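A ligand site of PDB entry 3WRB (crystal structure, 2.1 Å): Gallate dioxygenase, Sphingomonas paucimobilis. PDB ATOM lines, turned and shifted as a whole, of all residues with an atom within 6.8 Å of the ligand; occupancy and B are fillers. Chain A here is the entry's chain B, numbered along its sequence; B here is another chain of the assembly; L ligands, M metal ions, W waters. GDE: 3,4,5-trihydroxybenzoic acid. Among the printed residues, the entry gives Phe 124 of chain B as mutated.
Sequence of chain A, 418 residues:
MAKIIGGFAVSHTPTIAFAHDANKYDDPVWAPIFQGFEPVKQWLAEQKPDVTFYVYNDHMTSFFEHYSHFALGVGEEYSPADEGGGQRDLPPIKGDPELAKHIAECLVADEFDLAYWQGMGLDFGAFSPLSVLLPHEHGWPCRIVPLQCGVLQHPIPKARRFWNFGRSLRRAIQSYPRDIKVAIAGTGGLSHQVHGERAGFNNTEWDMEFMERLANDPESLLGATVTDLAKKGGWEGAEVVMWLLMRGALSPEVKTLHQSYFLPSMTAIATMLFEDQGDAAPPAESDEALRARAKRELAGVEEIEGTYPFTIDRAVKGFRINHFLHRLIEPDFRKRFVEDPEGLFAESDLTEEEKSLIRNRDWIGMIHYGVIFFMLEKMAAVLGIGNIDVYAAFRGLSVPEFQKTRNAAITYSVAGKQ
Water W2 bridges OAC of the ligand (2.6 Å) and N of Thr 13 of chain B (3.2 Å). Water W1 bridges an oxygen (OAE) of the ligand (2.7 Å) and a ring nitrogen (NE2) of His 192 of chain B (2.9 Å). Water W3 lies within hydrogen-bond range of the side-chain carboxylate (OE2) of Glu 239 of chain B and an oxygen (OAE) of the ligand.
Phe 373 touches the ligand. Phe 374 touches the ligand (CE1 to OAD, 3.7 Å). OG1 of Thr 13 of chain B touches CAF of the ligand, at 3.5 Å. CD of Pro 14 of chain B touches CAJ of the ligand, at 3.5 Å. Thr 15 of chain B touches the ligand. CZ of Phe 124 of chain B touches OAD of the ligand (3.5 Å). CG1 of Val 194 of chain B touches CAF of the ligand, at 3.9 Å. CB of Met 266 of chain B touches OAA of the ligand (3.6 Å). Of the 24 residues printed, 13 come within 4 Å of the ligand. The nearest printed residue that does not touch the ligand is His 59 of chain B (4.4 Å).
An oxygen (OAD) of the ligand lies within hydrogen-bond range of the side-chain carboxylate (OE2) of Glu 377. The side-chain hydroxyl of Tyr 391 is in hydrogen-bond range of an oxygen (OAB) of the ligand. OG1 of Thr 267 of chain B is in hydrogen-bond range of OAC of the ligand, at 2.8 Å. The side-chain amide nitrogen (ND2) of Asn 387 lies within hydrogen-bond range of an oxygen (OAB) of the ligand (2.9 Å). A ring nitrogen (NE2) of His 192 of chain B sits close to an oxygen (OAC) of the ligand, 3.2 Å away.
OE2 of Glu 377 sits at hydrogen-bond distance from ND2 of Asn 387 (3.4 Å). OG1 of Thr 13 of chain B sits at hydrogen-bond distance from OG1 of Thr 15 of chain B, 3.1 Å away. The backbone NH of Val 194 of chain B sits at hydrogen-bond distance from the side-chain carboxylate of Glu 236 of chain B (3.0 Å).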
ATOM      1  N   PHE A 373     -20.869 -36.022   6.617  1.00  0.00           N
ATOM      2  CA  PHE A 373     -21.598 -35.007   7.415  1.00  0.00           C
ATOM      3  C   PHE A 373     -21.566 -33.604   6.802  1.00  0.00           C
ATOM      4  O   PHE A 373     -22.555 -32.871   6.869  1.00  0.00           O
ATOM      5  CB  PHE A 373     -21.092 -34.906   8.871  1.00  0.00           C
ATOM      6  CG  PHE A 373     -21.673 -33.706   9.608  1.00  0.00           C
ATOM      7  CD1 PHE A 373     -23.011 -33.672   9.979  1.00  0.00           C
ATOM      8  CD2 PHE A 373     -20.877 -32.585   9.863  1.00  0.00           C
ATOM      9  CE1 PHE A 373     -23.572 -32.547  10.622  1.00  0.00           C
ATOM     10  CE2 PHE A 373     -21.417 -31.466  10.510  1.00  0.00           C
ATOM     11  CZ  PHE A 373     -22.782 -31.450  10.879  1.00  0.00           C
ATOM     12  N   PHE A 374     -20.442 -33.213   6.216  1.00  0.00           N
ATOM     13  CA  PHE A 374     -20.318 -31.840   5.696  1.00  0.00           C
ATOM     14  C   PHE A 374     -21.250 -31.514   4.534  1.00  0.00           C
ATOM     15  O   PHE A 374     -21.553 -30.345   4.288  1.00  0.00           O
ATOM     16  CB  PHE A 374     -18.844 -31.488   5.456  1.00  0.00           C
ATOM     17  CG  PHE A 374     -18.010 -31.694   6.669  1.00  0.00           C
ATOM     18  CD1 PHE A 374     -18.156 -30.844   7.784  1.00  0.00           C
ATOM     19  CD2 PHE A 374     -17.143 -32.766   6.772  1.00  0.00           C
ATOM     20  CE1 PHE A 374     -17.413 -31.045   8.942  1.00  0.00           C
ATOM     21  CE2 PHE A 374     -16.385 -32.984   7.930  1.00  0.00           C
ATOM     22  CZ  PHE A 374     -16.525 -32.114   9.009  1.00  0.00           C
ATOM     23  N   GLU A 377     -24.679 -30.991   6.540  1.00  0.00           N
ATOM     24  CA  GLU A 377     -24.563 -29.621   7.070  1.00  0.00           C
ATOM     25  C   GLU A 377     -25.034 -28.571   6.054  1.00  0.00           C
ATOM     26  O   GLU A 377     -25.712 -27.604   6.425  1.00  0.00           O
ATOM     27  CB  GLU A 377     -23.115 -29.378   7.498  1.00  0.00           C
ATOM     28  CG  GLU A 377     -22.758 -27.946   7.847  1.00  0.00           C
ATOM     29  CD  GLU A 377     -21.384 -27.845   8.467  1.00  0.00           C
ATOM     30  OE1 GLU A 377     -20.385 -28.118   7.760  1.00  0.00           O
ATOM     31  OE2 GLU A 377     -21.311 -27.494   9.678  1.00  0.00           O
ATOM     32  N   ASN A 387     -28.066 -27.568  12.930  1.00  0.00           N
ATOM     33  CA  ASN A 387     -27.238 -28.759  13.141  1.00  0.00           C
ATOM     34  C   ASN A 387     -27.672 -29.583  14.356  1.00  0.00           C
ATOM     35  O   ASN A 387     -27.491 -30.804  14.393  1.00  0.00           O
ATOM     36  CB  ASN A 387     -25.763 -28.370  13.267  1.00  0.00           C
ATOM     37  CG  ASN A 387     -25.092 -28.066  11.927  1.00  0.00           C
ATOM     38  OD1 ASN A 387     -25.694 -28.187  10.857  1.00  0.00           O
ATOM     39  ND2 ASN A 387     -23.815 -27.658  11.986  1.00  0.00           N
ATOM     40  N   ILE A 388     -28.275 -28.914  15.340  1.00  0.00           N
ATOM     41  CA  ILE A 388     -28.703 -29.560  16.574  1.00  0.00           C
ATOM     42  C   ILE A 388     -29.741 -30.663  16.309  1.00  0.00           C
ATOM     43  O   ILE A 388     -29.666 -31.740  16.890  1.00  0.00           O
ATOM     44  CB  ILE A 388     -29.252 -28.545  17.628  1.00  0.00           C
ATOM     45  CG1 ILE A 388     -28.418 -27.237  17.673  1.00  0.00           C
ATOM     46  CG2 ILE A 388     -29.377 -29.208  18.991  1.00  0.00           C
ATOM     47  CD1 ILE A 388     -26.888 -27.391  18.034  1.00  0.00           C
ATOM     48  N   TYR A 391     -27.869 -33.727  14.690  1.00  0.00           N
ATOM     49  CA  TYR A 391     -27.164 -34.479  15.730  1.00  0.00           C
ATOM     50  C   TYR A 391     -28.096 -35.313  16.624  1.00  0.00           C
ATOM     51  O   TYR A 391     -27.767 -36.459  16.986  1.00  0.00           O
ATOM     52  CB  TYR A 391     -26.348 -33.532  16.625  1.00  0.00           C
ATOM     53  CG  TYR A 391     -25.328 -32.664  15.902  1.00  0.00           C
ATOM     54  CD1 TYR A 391     -24.505 -33.188  14.896  1.00  0.00           C
ATOM     55  CD2 TYR A 391     -25.152 -31.328  16.268  1.00  0.00           C
ATOM     56  CE1 TYR A 391     -23.568 -32.391  14.250  1.00  0.00           C
ATOM     57  CE2 TYR A 391     -24.208 -30.531  15.635  1.00  0.00           C
ATOM     58  CZ  TYR A 391     -23.427 -31.063  14.619  1.00  0.00           C
ATOM     59  OH  TYR A 391     -22.489 -30.290  13.988  1.00  0.00           O
ATOM     60  N   TYR A 412     -27.795 -21.842  16.848  1.00  0.00           N
ATOM     61  CA  TYR A 412     -26.916 -21.500  15.717  1.00  0.00           C
ATOM     62  C   TYR A 412     -27.705 -21.465  14.401  1.00  0.00           C
ATOM     63  O   TYR A 412     -27.157 -21.188  13.331  1.00  0.00           O
ATOM     64  CB  TYR A 412     -25.759 -22.501  15.611  1.00  0.00           C
ATOM     65  N   HIS B  12     -11.660 -24.112  14.803  1.00  0.00           N
ATOM     66  CA  HIS B  12     -12.284 -23.399  13.684  1.00  0.00           C
ATOM     67  C   HIS B  12     -13.754 -23.700  13.444  1.00  0.00           C
ATOM     68  O   HIS B  12     -14.295 -23.295  12.414  1.00  0.00           O
ATOM     69  CB  HIS B  12     -11.456 -23.449  12.382  1.00  0.00           C
ATOM     70  CG  HIS B  12     -11.260 -24.807  11.798  1.00  0.00           C
ATOM     71  ND1 HIS B  12     -10.081 -25.181  11.173  1.00  0.00           N
ATOM     72  CD2 HIS B  12     -12.089 -25.881  11.702  1.00  0.00           C
ATOM     73  CE1 HIS B  12     -10.190 -26.423  10.740  1.00  0.00           C
ATOM     74  NE2 HIS B  12     -11.392 -26.872  11.051  1.00  0.00           N
ATOM     75  N   THR B  13     -14.412 -24.352  14.400  1.00  0.00           N
ATOM     76  CA  THR B  13     -15.849 -24.626  14.322  1.00  0.00           C
ATOM     77  C   THR B  13     -16.641 -23.392  13.873  1.00  0.00           C
ATOM     78  O   THR B  13     -16.357 -22.270  14.318  1.00  0.00           O
ATOM     79  CB  THR B  13     -16.447 -25.170  15.662  1.00  0.00           C
ATOM     80  OG1 THR B  13     -17.874 -25.041  15.616  1.00  0.00           O
ATOM     81  CG2 THR B  13     -15.933 -24.383  16.867  1.00  0.00           C
ATOM     82  N   PRO B  14     -17.652 -23.607  12.998  1.00  0.00           N
ATOM     83  CA  PRO B  14     -18.428 -22.509  12.423  1.00  0.00           C
ATOM     84  C   PRO B  14     -19.230 -21.695  13.450  1.00  0.00           C
ATOM     85  O   PRO B  14     -19.690 -20.608  13.119  1.00  0.00           O
ATOM     86  CB  PRO B  14     -19.388 -23.226  11.462  1.00  0.00           C
ATOM     87  CG  PRO B  14     -19.527 -24.596  12.015  1.00  0.00           C
ATOM     88  CD  PRO B  14     -18.168 -24.925  12.572  1.00  0.00           C
ATOM     89  N   THR B  15     -19.380 -22.223  14.669  1.00  0.00           N
ATOM     90  CA  THR B  15     -20.175 -21.563  15.745  1.00  0.00           C
ATOM     91  C   THR B  15     -19.531 -20.258  16.221  1.00  0.00           C
ATOM     92  O   THR B  15     -20.229 -19.321  16.586  1.00  0.00           O
ATOM     93  CB  THR B  15     -20.434 -22.495  16.963  1.00  0.00           C
ATOM     94  OG1 THR B  15     -19.198 -22.952  17.512  1.00  0.00           O
ATOM     95  CG2 THR B  15     -21.282 -23.697  16.557  1.00  0.00           C
ATOM     96  N   PHE B  18     -20.746 -17.651  13.920  1.00  0.00           N
ATOM     97  CA  PHE B  18     -22.169 -17.387  14.143  1.00  0.00           C
ATOM     98  C   PHE B  18     -22.339 -16.516  15.386  1.00  0.00           C
ATOM     99  O   PHE B  18     -23.131 -15.574  15.390  1.00  0.00           O
ATOM    100  CB  PHE B  18     -22.985 -18.689  14.307  1.00  0.00           C
ATOM    101  CG  PHE B  18     -22.883 -19.653  13.132  1.00  0.00           C
ATOM    102  CD1 PHE B  18     -23.016 -21.025  13.333  1.00  0.00           C
ATOM    103  CD2 PHE B  18     -22.672 -19.192  11.828  1.00  0.00           C
ATOM    104  CE1 PHE B  18     -22.939 -21.933  12.263  1.00  0.00           C
ATOM    105  CE2 PHE B  18     -22.581 -20.087  10.751  1.00  0.00           C
ATOM    106  CZ  PHE B  18     -22.722 -21.455  10.972  1.00  0.00           C
ATOM    107  N   HIS B  59     -14.228 -27.937   4.392  1.00  0.00           N
ATOM    108  CA  HIS B  59     -15.240 -28.888   4.848  1.00  0.00           C
ATOM    109  C   HIS B  59     -16.149 -29.251   3.692  1.00  0.00           C
ATOM    110  O   HIS B  59     -17.351 -28.956   3.670  1.00  0.00           O
ATOM    111  CB  HIS B  59     -15.962 -28.362   6.105  1.00  0.00           C
ATOM    112  CG  HIS B  59     -15.025 -28.143   7.258  1.00  0.00           C
ATOM    113  ND1 HIS B  59     -14.234 -27.026   7.385  1.00  0.00           N
ATOM    114  CD2 HIS B  59     -14.708 -28.942   8.311  1.00  0.00           C
ATOM    115  CE1 HIS B  59     -13.502 -27.126   8.480  1.00  0.00           C
ATOM    116  NE2 HIS B  59     -13.764 -28.288   9.052  1.00  0.00           N
ATOM    117  N   PHE B 124     -15.440 -21.800   6.259  1.00  0.00           N
ATOM    118  CA  PHE B 124     -15.376 -21.474   7.685  1.00  0.00           C
ATOM    119  C   PHE B 124     -14.099 -21.921   8.407  1.00  0.00           C
ATOM    120  O   PHE B 124     -13.757 -21.358   9.449  1.00  0.00           O
ATOM    121  CB  PHE B 124     -16.640 -21.933   8.437  1.00  0.00           C
ATOM    122  CG  PHE B 124     -16.739 -23.436   8.614  1.00  0.00           C
ATOM    123  CD1 PHE B 124     -15.995 -24.101   9.603  1.00  0.00           C
ATOM    124  CD2 PHE B 124     -17.637 -24.178   7.837  1.00  0.00           C
ATOM    125  CE1 PHE B 124     -16.114 -25.483   9.787  1.00  0.00           C
ATOM    126  CE2 PHE B 124     -17.770 -25.549   8.013  1.00  0.00           C
ATOM    127  CZ  PHE B 124     -17.012 -26.202   8.995  1.00  0.00           C
ATOM    128  N   GLY B 189     -10.071 -28.680  15.760  1.00  0.00           N
ATOM    129  CA  GLY B 189     -10.035 -29.282  17.091  1.00  0.00           C
ATOM    130  C   GLY B 189     -10.878 -28.486  18.092  1.00  0.00           C
ATOM    131  O   GLY B 189     -11.579 -27.546  17.713  1.00  0.00           O
ATOM    132  N   LEU B 190     -10.837 -28.870  19.371  1.00  0.00           N
ATOM    133  CA  LEU B 190     -10.181 -30.084  19.848  1.00  0.00           C
ATOM    134  C   LEU B 190     -11.170 -31.229  19.766  1.00  0.00           C
ATOM    135  O   LEU B 190     -11.797 -31.428  18.708  1.00  0.00           O
ATOM    136  CB  LEU B 190      -9.609 -29.890  21.261  1.00  0.00           C
ATOM    137  CG  LEU B 190      -8.384 -28.966  21.350  1.00  0.00           C
ATOM    138  CD1 LEU B 190      -7.937 -28.827  22.815  1.00  0.00           C
ATOM    139  CD2 LEU B 190      -7.224 -29.467  20.496  1.00  0.00           C
ATOM    140  N   HIS B 192     -14.143 -33.662  19.377  1.00  0.00           N
ATOM    141  CA  HIS B 192     -15.533 -33.618  18.925  1.00  0.00           C
ATOM    142  C   HIS B 192     -15.810 -34.712  17.910  1.00  0.00           C
ATOM    143  O   HIS B 192     -14.877 -35.278  17.311  1.00  0.00           O
ATOM    144  CB  HIS B 192     -15.932 -32.248  18.349  1.00  0.00           C
ATOM    145  CG  HIS B 192     -15.312 -31.912  17.023  1.00  0.00           C
ATOM    146  ND1 HIS B 192     -13.978 -31.613  16.892  1.00  0.00           N
ATOM    147  CD2 HIS B 192     -15.857 -31.814  15.783  1.00  0.00           C
ATOM    148  CE1 HIS B 192     -13.717 -31.332  15.620  1.00  0.00           C
ATOM    149  NE2 HIS B 192     -14.835 -31.452  14.928  1.00  0.00           N
ATOM    150  N   GLN B 193     -17.090 -35.002  17.718  1.00  0.00           N
ATOM    151  CA  GLN B 193     -17.545 -35.889  16.671  1.00  0.00           C
ATOM    152  C   GLN B 193     -18.911 -35.426  16.220  1.00  0.00           C
ATOM    153  O   GLN B 193     -19.829 -35.271  17.040  1.00  0.00           O
ATOM    154  CB  GLN B 193     -17.571 -37.363  17.117  1.00  0.00           C
ATOM    155  CG  GLN B 193     -18.016 -38.301  15.974  1.00  0.00           C
ATOM    156  CD  GLN B 193     -17.543 -39.752  16.108  1.00  0.00           C
ATOM    157  OE1 GLN B 193     -16.512 -40.059  16.720  1.00  0.00           O
ATOM    158  NE2 GLN B 193     -18.302 -40.649  15.515  1.00  0.00           N
ATOM    159  N   VAL B 194     -19.043 -35.200  14.906  1.00  0.00           N
ATOM    160  CA  VAL B 194     -20.259 -34.587  14.367  1.00  0.00           C
ATOM    161  C   VAL B 194     -21.091 -35.493  13.458  1.00  0.00           C
ATOM    162  O   VAL B 194     -22.043 -35.037  12.839  1.00  0.00           O
ATOM    163  CB  VAL B 194     -19.970 -33.207  13.649  1.00  0.00           C
ATOM    164  CG1 VAL B 194     -19.707 -32.120  14.680  1.00  0.00           C
ATOM    165  CG2 VAL B 194     -18.824 -33.322  12.613  1.00  0.00           C
ATOM    166  N   GLU B 236     -13.847 -36.511  13.984  1.00  0.00           N
ATOM    167  CA  GLU B 236     -13.428 -35.238  13.409  1.00  0.00           C
ATOM    168  C   GLU B 236     -12.380 -34.551  14.263  1.00  0.00           C
ATOM    169  O   GLU B 236     -11.565 -33.767  13.750  1.00  0.00           O
ATOM    170  CB  GLU B 236     -14.645 -34.357  13.139  1.00  0.00           C
ATOM    171  CG  GLU B 236     -15.504 -34.866  11.958  1.00  0.00           C
ATOM    172  CD  GLU B 236     -16.473 -35.973  12.336  1.00  0.00           C
ATOM    173  OE1 GLU B 236     -16.567 -36.324  13.529  1.00  0.00           O
ATOM    174  OE2 GLU B 236     -17.173 -36.485  11.423  1.00  0.00           O
ATOM    175  N   GLU B 239      -8.569 -34.216  13.530  1.00  0.00           N
ATOM    176  CA  GLU B 239      -7.994 -33.169  12.690  1.00  0.00           C
ATOM    177  C   GLU B 239      -6.849 -32.412  13.410  1.00  0.00           C
ATOM    178  O   GLU B 239      -6.140 -31.597  12.779  1.00  0.00           O
ATOM    179  CB  GLU B 239      -9.077 -32.198  12.169  1.00  0.00           C
ATOM    180  CG  GLU B 239      -9.597 -31.205  13.214  1.00  0.00           C
ATOM    181  CD  GLU B 239     -10.678 -30.287  12.715  1.00  0.00           C
ATOM    182  OE1 GLU B 239     -10.688 -29.975  11.506  1.00  0.00           O
ATOM    183  OE2 GLU B 239     -11.530 -29.845  13.523  1.00  0.00           O
ATOM    184  N   SER B 265     -21.035 -26.675  23.752  1.00  0.00           N
ATOM    185  CA  SER B 265     -21.907 -27.475  22.894  1.00  0.00           C
ATOM    186  C   SER B 265     -21.159 -28.681  22.297  1.00  0.00           C
ATOM    187  O   SER B 265     -20.699 -29.548  23.034  1.00  0.00           O
ATOM    188  CB  SER B 265     -22.532 -26.596  21.813  1.00  0.00           C
ATOM    189  OG  SER B 265     -23.553 -27.304  21.138  1.00  0.00           O
ATOM    190  N   MET B 266     -21.017 -28.726  20.975  1.00  0.00           N
ATOM    191  CA  MET B 266     -20.418 -29.899  20.293  1.00  0.00           C
ATOM    192  C   MET B 266     -18.892 -30.001  20.350  1.00  0.00           C
ATOM    193  O   MET B 266     -18.350 -31.101  20.481  1.00  0.00           O
ATOM    194  CB  MET B 266     -20.889 -29.958  18.836  1.00  0.00           C
ATOM    195  CG  MET B 266     -22.387 -30.132  18.681  1.00  0.00           C
ATOM    196  SD  MET B 266     -23.025 -31.743  19.222  1.00  0.00           S
ATOM    197  CE  MET B 266     -22.068 -32.862  18.179  1.00  0.00           C
ATOM    198  N   THR B 267     -18.205 -28.860  20.269  1.00  0.00           N
ATOM    199  CA  THR B 267     -16.752 -28.834  20.055  1.00  0.00           C
ATOM    200  C   THR B 267     -15.979 -28.104  21.153  1.00  0.00           C
ATOM    201  O   THR B 267     -16.353 -26.993  21.577  1.00  0.00           O
ATOM    202  CB  THR B 267     -16.416 -28.140  18.705  1.00  0.00           C
ATOM    203  OG1 THR B 267     -17.144 -28.790  17.664  1.00  0.00           O
ATOM    204  CG2 THR B 267     -14.915 -28.205  18.396  1.00  0.00           C
HETATM  205  OAA GDE L   1     -21.292 -27.383  16.330  1.00  0.00           O
HETATM  206  OAB GDE L   1     -22.615 -27.651  14.614  1.00  0.00           O
HETATM  207  OAC GDE L   1     -16.720 -28.839  14.918  1.00  0.00           O
HETATM  208  OAD GDE L   1     -19.120 -28.283  10.816  1.00  0.00           O
HETATM  209  OAE GDE L   1     -16.813 -28.851  12.140  1.00  0.00           O
HETATM  210  CAF GDE L   1     -19.046 -28.263  14.969  1.00  0.00           C
HETATM  211  CAG GDE L   1     -20.282 -27.969  12.906  1.00  0.00           C
HETATM  212  CAH GDE L   1     -21.469 -27.647  15.131  1.00  0.00           C
HETATM  213  CAI GDE L   1     -17.890 -28.558  14.246  1.00  0.00           C
HETATM  214  CAJ GDE L   1     -19.119 -28.274  12.178  1.00  0.00           C
HETATM  215  CAK GDE L   1     -20.239 -27.967  14.309  1.00  0.00           C
HETATM  216  CAL GDE L   1     -17.927 -28.560  12.855  1.00  0.00           C
HETATM  217 FE    FE M   1     -12.136 -28.902  10.446  1.00  0.00          FE
HETATM  218  O   HOH W   1     -15.099 -30.923  12.052  1.00  0.00           O
HETATM  219  O   HOH W   2     -14.679 -27.510  14.141  1.00  0.00           O
HETATM  220  O   HOH W   3     -13.425 -28.933  12.085  1.00  0.00           O
